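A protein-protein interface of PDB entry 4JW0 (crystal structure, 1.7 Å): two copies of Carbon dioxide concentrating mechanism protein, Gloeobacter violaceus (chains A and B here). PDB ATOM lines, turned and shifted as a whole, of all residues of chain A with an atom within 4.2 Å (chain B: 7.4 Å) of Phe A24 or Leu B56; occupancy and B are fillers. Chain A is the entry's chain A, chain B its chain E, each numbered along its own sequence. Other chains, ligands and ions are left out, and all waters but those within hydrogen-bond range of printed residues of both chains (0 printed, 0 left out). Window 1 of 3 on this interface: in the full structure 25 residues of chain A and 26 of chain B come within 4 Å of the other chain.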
ATOM      1  N   THR A   9      18.422  -8.928  -2.450  1.00  0.00           N
ATOM      2  CA  THR A   9      18.762 -10.224  -1.905  1.00  0.00           C
ATOM      3  C   THR A   9      19.243 -11.150  -3.012  1.00  0.00           C
ATOM      4  O   THR A   9      18.866 -11.012  -4.176  1.00  0.00           O
ATOM      5  CB  THR A   9      17.557 -10.886  -1.212  1.00  0.00           C
ATOM      6  OG1 THR A   9      16.627 -11.335  -2.201  1.00  0.00           O
ATOM      7  CG2 THR A   9      16.872  -9.911  -0.280  1.00  0.00           C
ATOM      8  N   VAL A  10      20.084 -12.097  -2.626  1.00  0.00           N
ATOM      9  CA  VAL A  10      20.560 -13.122  -3.532  1.00  0.00           C
ATOM     10  C   VAL A  10      20.064 -14.463  -3.008  1.00  0.00           C
ATOM     11  O   VAL A  10      20.193 -14.753  -1.821  1.00  0.00           O
ATOM     12  CB  VAL A  10      22.088 -13.126  -3.606  1.00  0.00           C
ATOM     13  CG1 VAL A  10      22.573 -14.235  -4.520  1.00  0.00           C
ATOM     14  CG2 VAL A  10      22.595 -11.772  -4.093  1.00  0.00           C
ATOM     15  N   MET A  19      26.266 -23.617   4.148  1.00  0.00           N
ATOM     16  CA  MET A  19      25.708 -22.284   3.932  1.00  0.00           C
ATOM     17  C   MET A  19      24.185 -22.239   3.945  1.00  0.00           C
ATOM     18  O   MET A  19      23.601 -21.170   3.813  1.00  0.00           O
ATOM     19  CB  MET A  19      26.213 -21.695   2.614  1.00  0.00           C
ATOM     20  CG  MET A  19      27.692 -21.343   2.608  1.00  0.00           C
ATOM     21  SD  MET A  19      28.158 -20.136   3.864  1.00  0.00           S
ATOM     22  CE  MET A  19      27.085 -18.761   3.443  1.00  0.00           C
ATOM     23  N   VAL A  22      21.583 -19.280   5.618  1.00  0.00           N
ATOM     24  CA  VAL A  22      22.176 -17.945   5.631  1.00  0.00           C
ATOM     25  C   VAL A  22      21.451 -17.023   4.659  1.00  0.00           C
ATOM     26  O   VAL A  22      21.311 -17.348   3.482  1.00  0.00           O
ATOM     27  CB  VAL A  22      23.668 -17.987   5.256  1.00  0.00           C
ATOM     28  CG1 VAL A  22      24.232 -16.575   5.183  1.00  0.00           C
ATOM     29  CG2 VAL A  22      24.449 -18.829   6.260  1.00  0.00           C
ATOM     30  N   LYS A  23      21.001 -15.868   5.150  1.00  0.00           N
ATOM     31  CA  LYS A  23      20.380 -14.868   4.293  1.00  0.00           C
ATOM     32  C   LYS A  23      21.453 -14.003   3.642  1.00  0.00           C
ATOM     33  O   LYS A  23      22.373 -13.541   4.313  1.00  0.00           O
ATOM     34  CB  LYS A  23      19.414 -13.977   5.077  1.00  0.00           C
ATOM     35  CG  LYS A  23      18.690 -12.975   4.179  1.00  0.00           C
ATOM     36  CD  LYS A  23      17.472 -12.356   4.835  1.00  0.00           C
ATOM     37  CE  LYS A  23      16.741 -11.454   3.845  1.00  0.00           C
ATOM     38  NZ  LYS A  23      15.663 -10.642   4.475  1.00  0.00           N
ATOM     39  N   PHE A  24      21.320 -13.798   2.336  1.00  0.00           N
ATOM     40  CA  PHE A  24      22.292 -13.050   1.546  1.00  0.00           C
ATOM     41  C   PHE A  24      21.733 -11.704   1.113  1.00  0.00           C
ATOM     42  O   PHE A  24      20.861 -11.641   0.247  1.00  0.00           O
ATOM     43  CB  PHE A  24      22.671 -13.839   0.291  1.00  0.00           C
ATOM     44  CG  PHE A  24      23.311 -15.167   0.573  1.00  0.00           C
ATOM     45  CD1 PHE A  24      24.391 -15.264   1.432  1.00  0.00           C
ATOM     46  CD2 PHE A  24      22.827 -16.319  -0.020  1.00  0.00           C
ATOM     47  CE1 PHE A  24      24.982 -16.483   1.688  1.00  0.00           C
ATOM     48  CE2 PHE A  24      23.412 -17.545   0.235  1.00  0.00           C
ATOM     49  CZ  PHE A  24      24.488 -17.626   1.096  1.00  0.00           C
ATOM     50  N   LEU A  25      22.256 -10.625   1.684  1.00  0.00           N
ATOM     51  CA  LEU A  25      21.847  -9.284   1.283  1.00  0.00           C
ATOM     52  C   LEU A  25      22.821  -8.684   0.282  1.00  0.00           C
ATOM     53  O   LEU A  25      24.039  -8.755   0.469  1.00  0.00           O
ATOM     54  CB  LEU A  25      21.759  -8.351   2.491  1.00  0.00           C
ATOM     55  CG  LEU A  25      20.663  -8.594   3.524  1.00  0.00           C
ATOM     56  CD1 LEU A  25      20.729  -7.513   4.601  1.00  0.00           C
ATOM     57  CD2 LEU A  25      19.289  -8.623   2.871  1.00  0.00           C
ATOM     58  N   LEU A  26      22.275  -8.091  -0.776  1.00  0.00           N
ATOM     59  CA  LEU A  26      23.059  -7.313  -1.717  1.00  0.00           C
ATOM     60  C   LEU A  26      23.227  -5.904  -1.164  1.00  0.00           C
ATOM     61  O   LEU A  26      22.255  -5.156  -1.044  1.00  0.00           O
ATOM     62  CB  LEU A  26      22.369  -7.251  -3.080  1.00  0.00           C
ATOM     63  CG  LEU A  26      23.092  -6.416  -4.136  1.00  0.00           C
ATOM     64  CD1 LEU A  26      24.515  -6.897  -4.298  1.00  0.00           C
ATOM     65  CD2 LEU A  26      22.362  -6.453  -5.467  1.00  0.00           C
ATOM     66  N   VAL A  42      27.941  -8.897  -1.120  1.00  0.00           N
ATOM     67  CA  VAL A  42      26.842  -9.757  -0.724  1.00  0.00           C
ATOM     68  C   VAL A  42      27.207 -10.301   0.645  1.00  0.00           C
ATOM     69  O   VAL A  42      28.219 -10.985   0.803  1.00  0.00           O
ATOM     70  CB  VAL A  42      26.595 -10.899  -1.724  1.00  0.00           C
ATOM     71  CG1 VAL A  42      25.420 -11.756  -1.257  1.00  0.00           C
ATOM     72  CG2 VAL A  42      26.327 -10.339  -3.110  1.00  0.00           C
ATOM     73  N   ALA A  43      26.391  -9.978   1.641  1.00  0.00           N
ATOM     74  CA  ALA A  43      26.745 -10.236   3.027  1.00  0.00           C
ATOM     75  C   ALA A  43      25.715 -11.098   3.729  1.00  0.00           C
ATOM     76  O   ALA A  43      24.517 -10.974   3.477  1.00  0.00           O
ATOM     77  CB  ALA A  43      26.896  -8.922   3.769  1.00  0.00           C
ATOM     78  N   MET B   1      30.865 -11.548   0.130  1.00  0.00           N
ATOM     79  CA  MET B   1      30.898 -12.384  -1.097  1.00  0.00           C
ATOM     80  C   MET B   1      30.694 -11.506  -2.323  1.00  0.00           C
ATOM     81  O   MET B   1      30.164 -10.404  -2.221  1.00  0.00           O
ATOM     82  CB  MET B   1      29.804 -13.458  -1.038  1.00  0.00           C
ATOM     83  CG  MET B   1      30.090 -14.584  -0.055  1.00  0.00           C
ATOM     84  SD  MET B   1      29.732 -14.160   1.661  1.00  0.00           S
ATOM     85  CE  MET B   1      27.938 -14.127   1.666  1.00  0.00           C
ATOM     86  N   GLN B   2      31.118 -12.000  -3.478  1.00  0.00           N
ATOM     87  CA  GLN B   2      30.867 -11.322  -4.742  1.00  0.00           C
ATOM     88  C   GLN B   2      30.109 -12.250  -5.682  1.00  0.00           C
ATOM     89  O   GLN B   2      30.046 -13.462  -5.467  1.00  0.00           O
ATOM     90  CB  GLN B   2      32.179 -10.887  -5.405  1.00  0.00           C
ATOM     91  CG  GLN B   2      33.030  -9.941  -4.563  1.00  0.00           C
ATOM     92  CD  GLN B   2      32.514  -8.519  -4.584  1.00  0.00           C
ATOM     93  OE1 GLN B   2      32.798  -7.758  -5.506  1.00  0.00           O
ATOM     94  NE2 GLN B   2      31.754  -8.154  -3.567  1.00  0.00           N
ATOM     95  N   ILE B   3      29.523 -11.658  -6.714  1.00  0.00           N
ATOM     96  CA  ILE B   3      28.891 -12.406  -7.786  1.00  0.00           C
ATOM     97  C   ILE B   3      29.878 -12.565  -8.936  1.00  0.00           C
ATOM     98  O   ILE B   3      30.506 -11.599  -9.378  1.00  0.00           O
ATOM     99  CB  ILE B   3      27.636 -11.676  -8.306  1.00  0.00           C
ATOM    100  CG1 ILE B   3      26.633 -11.474  -7.169  1.00  0.00           C
ATOM    101  CG2 ILE B   3      27.007 -12.453  -9.458  1.00  0.00           C
ATOM    102  CD1 ILE B   3      25.572 -10.442  -7.475  1.00  0.00           C
ATOM    103  N   GLY B   4      30.020 -13.793  -9.410  1.00  0.00           N
ATOM    104  CA  GLY B   4      30.835 -14.060 -10.571  1.00  0.00           C
ATOM    105  C   GLY B   4      30.070 -14.873 -11.593  1.00  0.00           C
ATOM    106  O   GLY B   4      29.113 -15.580 -11.265  1.00  0.00           O
ATOM    107  N   LEU B  27      36.227 -17.207 -12.979  1.00  0.00           N
ATOM    108  CA  LEU B  27      35.037 -16.413 -12.754  1.00  0.00           C
ATOM    109  C   LEU B  27      35.259 -15.000 -13.237  1.00  0.00           C
ATOM    110  O   LEU B  27      36.292 -14.397 -12.955  1.00  0.00           O
ATOM    111  CB  LEU B  27      34.703 -16.365 -11.263  1.00  0.00           C
ATOM    112  CG  LEU B  27      34.503 -17.699 -10.551  1.00  0.00           C
ATOM    113  CD1 LEU B  27      34.125 -17.446  -9.109  1.00  0.00           C
ATOM    114  CD2 LEU B  27      33.444 -18.530 -11.265  1.00  0.00           C
ATOM    115  N   ALA B  43      38.516 -19.760  -8.715  1.00  0.00           N
ATOM    116  CA  ALA B  43      37.983 -20.266  -7.457  1.00  0.00           C
ATOM    117  C   ALA B  43      37.859 -21.775  -7.457  1.00  0.00           C
ATOM    118  O   ALA B  43      37.593 -22.385  -8.492  1.00  0.00           O
ATOM    119  CB  ALA B  43      36.614 -19.647  -7.186  1.00  0.00           C
ATOM    120  N   TRP B  54      25.760 -17.907 -12.825  1.00  0.00           N
ATOM    121  CA  TRP B  54      26.202 -16.938 -11.836  1.00  0.00           C
ATOM    122  C   TRP B  54      26.431 -17.662 -10.523  1.00  0.00           C
ATOM    123  O   TRP B  54      25.649 -18.543 -10.139  1.00  0.00           O
ATOM    124  CB  TRP B  54      25.166 -15.844 -11.620  1.00  0.00           C
ATOM    125  CG  TRP B  54      25.092 -14.844 -12.718  1.00  0.00           C
ATOM    126  CD1 TRP B  54      25.512 -15.003 -14.012  1.00  0.00           C
ATOM    127  CD2 TRP B  54      24.574 -13.516 -12.617  1.00  0.00           C
ATOM    128  NE1 TRP B  54      25.275 -13.849 -14.725  1.00  0.00           N
ATOM    129  CE2 TRP B  54      24.706 -12.925 -13.899  1.00  0.00           C
ATOM    130  CE3 TRP B  54      24.008 -12.770 -11.582  1.00  0.00           C
ATOM    131  CZ2 TRP B  54      24.286 -11.622 -14.154  1.00  0.00           C
ATOM    132  CZ3 TRP B  54      23.594 -11.478 -11.844  1.00  0.00           C
ATOM    133  CH2 TRP B  54      23.737 -10.918 -13.123  1.00  0.00           C
ATOM    134  N   VAL B  55      27.496 -17.289  -9.834  1.00  0.00           N
ATOM    135  CA  VAL B  55      27.810 -17.900  -8.556  1.00  0.00           C
ATOM    136  C   VAL B  55      28.131 -16.843  -7.524  1.00  0.00           C
ATOM    137  O   VAL B  55      28.505 -15.720  -7.854  1.00  0.00           O
ATOM    138  CB  VAL B  55      29.000 -18.877  -8.655  1.00  0.00           C
ATOM    139  CG1 VAL B  55      28.698 -19.973  -9.664  1.00  0.00           C
ATOM    140  CG2 VAL B  55      30.272 -18.136  -9.033  1.00  0.00           C
ATOM    141  N   LEU B  56      27.945 -17.220  -6.271  1.00  0.00           N
ATOM    142  CA  LEU B  56      28.392 -16.442  -5.139  1.00  0.00           C
ATOM    143  C   LEU B  56      29.728 -17.055  -4.759  1.00  0.00           C
ATOM    144  O   LEU B  56      29.842 -18.282  -4.658  1.00  0.00           O
ATOM    145  CB  LEU B  56      27.377 -16.588  -4.006  1.00  0.00           C
ATOM    146  CG  LEU B  56      26.922 -15.422  -3.131  1.00  0.00           C
ATOM    147  CD1 LEU B  56      26.754 -14.136  -3.905  1.00  0.00           C
ATOM    148  CD2 LEU B  56      25.603 -15.824  -2.483  1.00  0.00           C
ATOM    149  N   PHE B  57      30.755 -16.228  -4.591  1.00  0.00           N
ATOM    150  CA  PHE B  57      32.043 -16.739  -4.155  1.00  0.00           C
ATOM    151  C   PHE B  57      32.634 -15.892  -3.041  1.00  0.00           C
ATOM    152  O   PHE B  57      32.351 -14.692  -2.929  1.00  0.00           O
ATOM    153  CB  PHE B  57      33.031 -16.902  -5.321  1.00  0.00           C
ATOM    154  CG  PHE B  57      33.540 -15.607  -5.909  1.00  0.00           C
ATOM    155  CD1 PHE B  57      32.836 -14.963  -6.921  1.00  0.00           C
ATOM    156  CD2 PHE B  57      34.745 -15.065  -5.496  1.00  0.00           C
ATOM    157  CE1 PHE B  57      33.311 -13.794  -7.485  1.00  0.00           C
ATOM    158  CE2 PHE B  57      35.225 -13.889  -6.053  1.00  0.00           C
ATOM    159  CZ  PHE B  57      34.510 -13.255  -7.050  1.00  0.00           C
ATOM    160  N   SER B  58      33.435 -16.552  -2.213  1.00  0.00           N
ATOM    161  CA  SER B  58      34.079 -15.938  -1.058  1.00  0.00           C
ATOM    162  C   SER B  58      35.570 -15.945  -1.254  1.00  0.00           C
ATOM    163  O   SER B  58      36.101 -16.810  -1.940  1.00  0.00           O
ATOM    164  CB  SER B  58      33.742 -16.711   0.214  1.00  0.00           C
ATOM    165  OG  SER B  58      32.380 -16.551   0.537  1.00  0.00           O
ATOM    166  N   VAL B  77      36.543 -19.480  -3.176  1.00  0.00           N
ATOM    167  CA  VAL B  77      35.676 -20.650  -3.221  1.00  0.00           C
ATOM    168  C   VAL B  77      34.280 -20.283  -3.710  1.00  0.00           C
ATOM    169  O   VAL B  77      33.725 -19.239  -3.336  1.00  0.00           O
ATOM    170  CB  VAL B  77      35.575 -21.319  -1.827  1.00  0.00           C
ATOM    171  CG1 VAL B  77      34.950 -20.371  -0.811  1.00  0.00           C
ATOM    172  CG2 VAL B  77      34.783 -22.616  -1.905  1.00  0.00           C
ATOM    173  N   VAL B  78      33.731 -21.136  -4.572  1.00  0.00           N
ATOM    174  CA  VAL B  78      32.343 -21.018  -4.993  1.00  0.00           C
ATOM    175  C   VAL B  78      31.482 -21.602  -3.886  1.00  0.00           C
ATOM    176  O   VAL B  78      31.665 -22.753  -3.507  1.00  0.00           O
ATOM    177  CB  VAL B  78      32.072 -21.818  -6.293  1.00  0.00           C
ATOM    178  CG1 VAL B  78      30.591 -21.786  -6.637  1.00  0.00           C
ATOM    179  CG2 VAL B  78      32.909 -21.281  -7.443  1.00  0.00           C
ATOM    180  N   ILE B  79      30.550 -20.819  -3.357  1.00  0.00           N
ATOM    181  CA  ILE B  79      29.710 -21.314  -2.272  1.00  0.00           C
ATOM    182  C   ILE B  79      28.287 -21.647  -2.718  1.00  0.00           C
ATOM    183  O   ILE B  79      27.555 -22.311  -1.990  1.00  0.00           O
ATOM    184  CB  ILE B  79      29.684 -20.346  -1.069  1.00  0.00           C
ATOM    185  CG1 ILE B  79      29.018 -19.021  -1.440  1.00  0.00           C
ATOM    186  CG2 ILE B  79      31.090 -20.116  -0.562  1.00  0.00           C
ATOM    187  CD1 ILE B  79      28.803 -18.106  -0.257  1.00  0.00           C
ATOM    188  N   GLY B  80      27.908 -21.210  -3.914  1.00  0.00           N
ATOM    189  CA  GLY B  80      26.594 -21.521  -4.445  1.00  0.00           C
ATOM    190  C   GLY B  80      26.357 -20.975  -5.839  1.00  0.00           C
ATOM    191  O   GLY B  80      26.947 -19.973  -6.234  1.00  0.00           O
ATOM    192  N   ILE B  81      25.492 -21.656  -6.585  1.00  0.00           N
ATOM    193  CA  ILE B  81      25.001 -21.169  -7.866  1.00  0.00           C
ATOM    194  C   ILE B  81      23.765 -20.316  -7.602  1.00  0.00           C
ATOM    195  O   ILE B  81      22.877 -20.712  -6.841  1.00  0.00           O
ATOM    196  CB  ILE B  81      24.620 -22.331  -8.820  1.00  0.00           C
ATOM    197  CG1 ILE B  81      25.865 -23.081  -9.303  1.00  0.00           C
ATOM    198  CG2 ILE B  81      23.865 -21.803 -10.026  1.00  0.00           C
ATOM    199  CD1 ILE B  81      26.624 -23.781  -8.223  1.00  0.00           C
ATOM    200  N   ILE B  82      23.703 -19.151  -8.235  1.00  0.00           N
ATOM    201  CA  ILE B  82      22.633 -18.194  -7.978  1.00  0.00           C
ATOM    202  C   ILE B  82      21.380 -18.493  -8.802  1.00  0.00           C
ATOM    203  O   ILE B  82      21.454 -18.723 -10.007  1.00  0.00           O
ATOM    204  CB  ILE B  82      23.111 -16.757  -8.261  1.00  0.00           C
ATOM    205  CG1 ILE B  82      24.189 -16.359  -7.245  1.00  0.00           C
ATOM    206  CG2 ILE B  82      21.942 -15.774  -8.219  1.00  0.00           C
ATOM    207  CD1 ILE B  82      24.923 -15.072  -7.591  1.00  0.00           C
ATOM    208  N   VAL B  85      18.689 -12.828  -8.287  1.00  0.00           N
ATOM    209  CA  VAL B  85      19.125 -11.612  -7.627  1.00  0.00           C
ATOM    210  C   VAL B  85      18.016 -10.592  -7.807  1.00  0.00           C
ATOM    211  O   VAL B  85      17.544 -10.370  -8.921  1.00  0.00           O
ATOM    212  CB  VAL B  85      20.414 -11.048  -8.232  1.00  0.00           C
ATOM    213  CG1 VAL B  85      20.854  -9.819  -7.459  1.00  0.00           C
ATOM    214  CG2 VAL B  85      21.509 -12.094  -8.242  1.00  0.00           C
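1 position is printed for both chains. Of the 7 pairs that touch across the chains among the printed residues, none has its exchanged pair printed and touching as well.
Phe A24 touches just these residues of chain B: Met B1 and Leu B56. Of the printed residues of chain A, Leu B56 touches Val A10, Phe A24 and Val A42. Of the printed residues of chain A, Val B85 touches Thr A9 (3.5 Å). Of the printed residues of chain B, Val A10 touches Leu B56 (3.98 Å) and Ile B82 (3.8 Å). Printed residues of chain B within 4 Å of Thr A9: Val B85 (3.5 Å). Ile B79 touches none of the printed residues of chain A. Val B77 touches none of the printed residues of chain A. The nearest residue of chain B that does not touch Phe A24 is Ile B79 (4.5 Å). The nearest printed residue of chain A that does not touch Met B1 is Ala A43 (4.3 Å).
Hydrophobic or aromatic side chains of chain A that line the printed part of chain B: Val A10, Phe A24 and Val A42. Hydrophobic or aromatic side chains of chain B within 4 Å of the printed part of chain A: Met B1, Leu B56 and Ile B82. Among the printed residues, 7 pairs touch across the chains.
SD of Met B1 lies close to OG of Ser B58, 3.7 Å away. The backbone carbonyl oxygen of Leu B56 lies within hydrogen-bond range of the backbone NH of Ile B79 (2.9 Å). The backbone carbonyl oxygen (O) of Gly B80 is in hydrogen-bond range of the backbone NH (N) of Leu B56, at 2.9 Å. O of Trp B54 sits at hydrogen-bond distance from N of Ile B82, at 2.8 Å. The backbone carbonyl oxygen of Phe A24 lies within hydrogen-bond range of the backbone NH of Val A10 (3.0 Å).
O of Val A42 is in hydrogen-bond range of N of Met B1, 2.8 Å away.
Among the printed residues, merely in contact across the chains: Thr A9 with Val B85, Val A10 with Leu B56, Val A10 with Ile B82, Phe A24 with Met B1, Phe A24 with Leu B56 and Val A42 with Leu B56.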
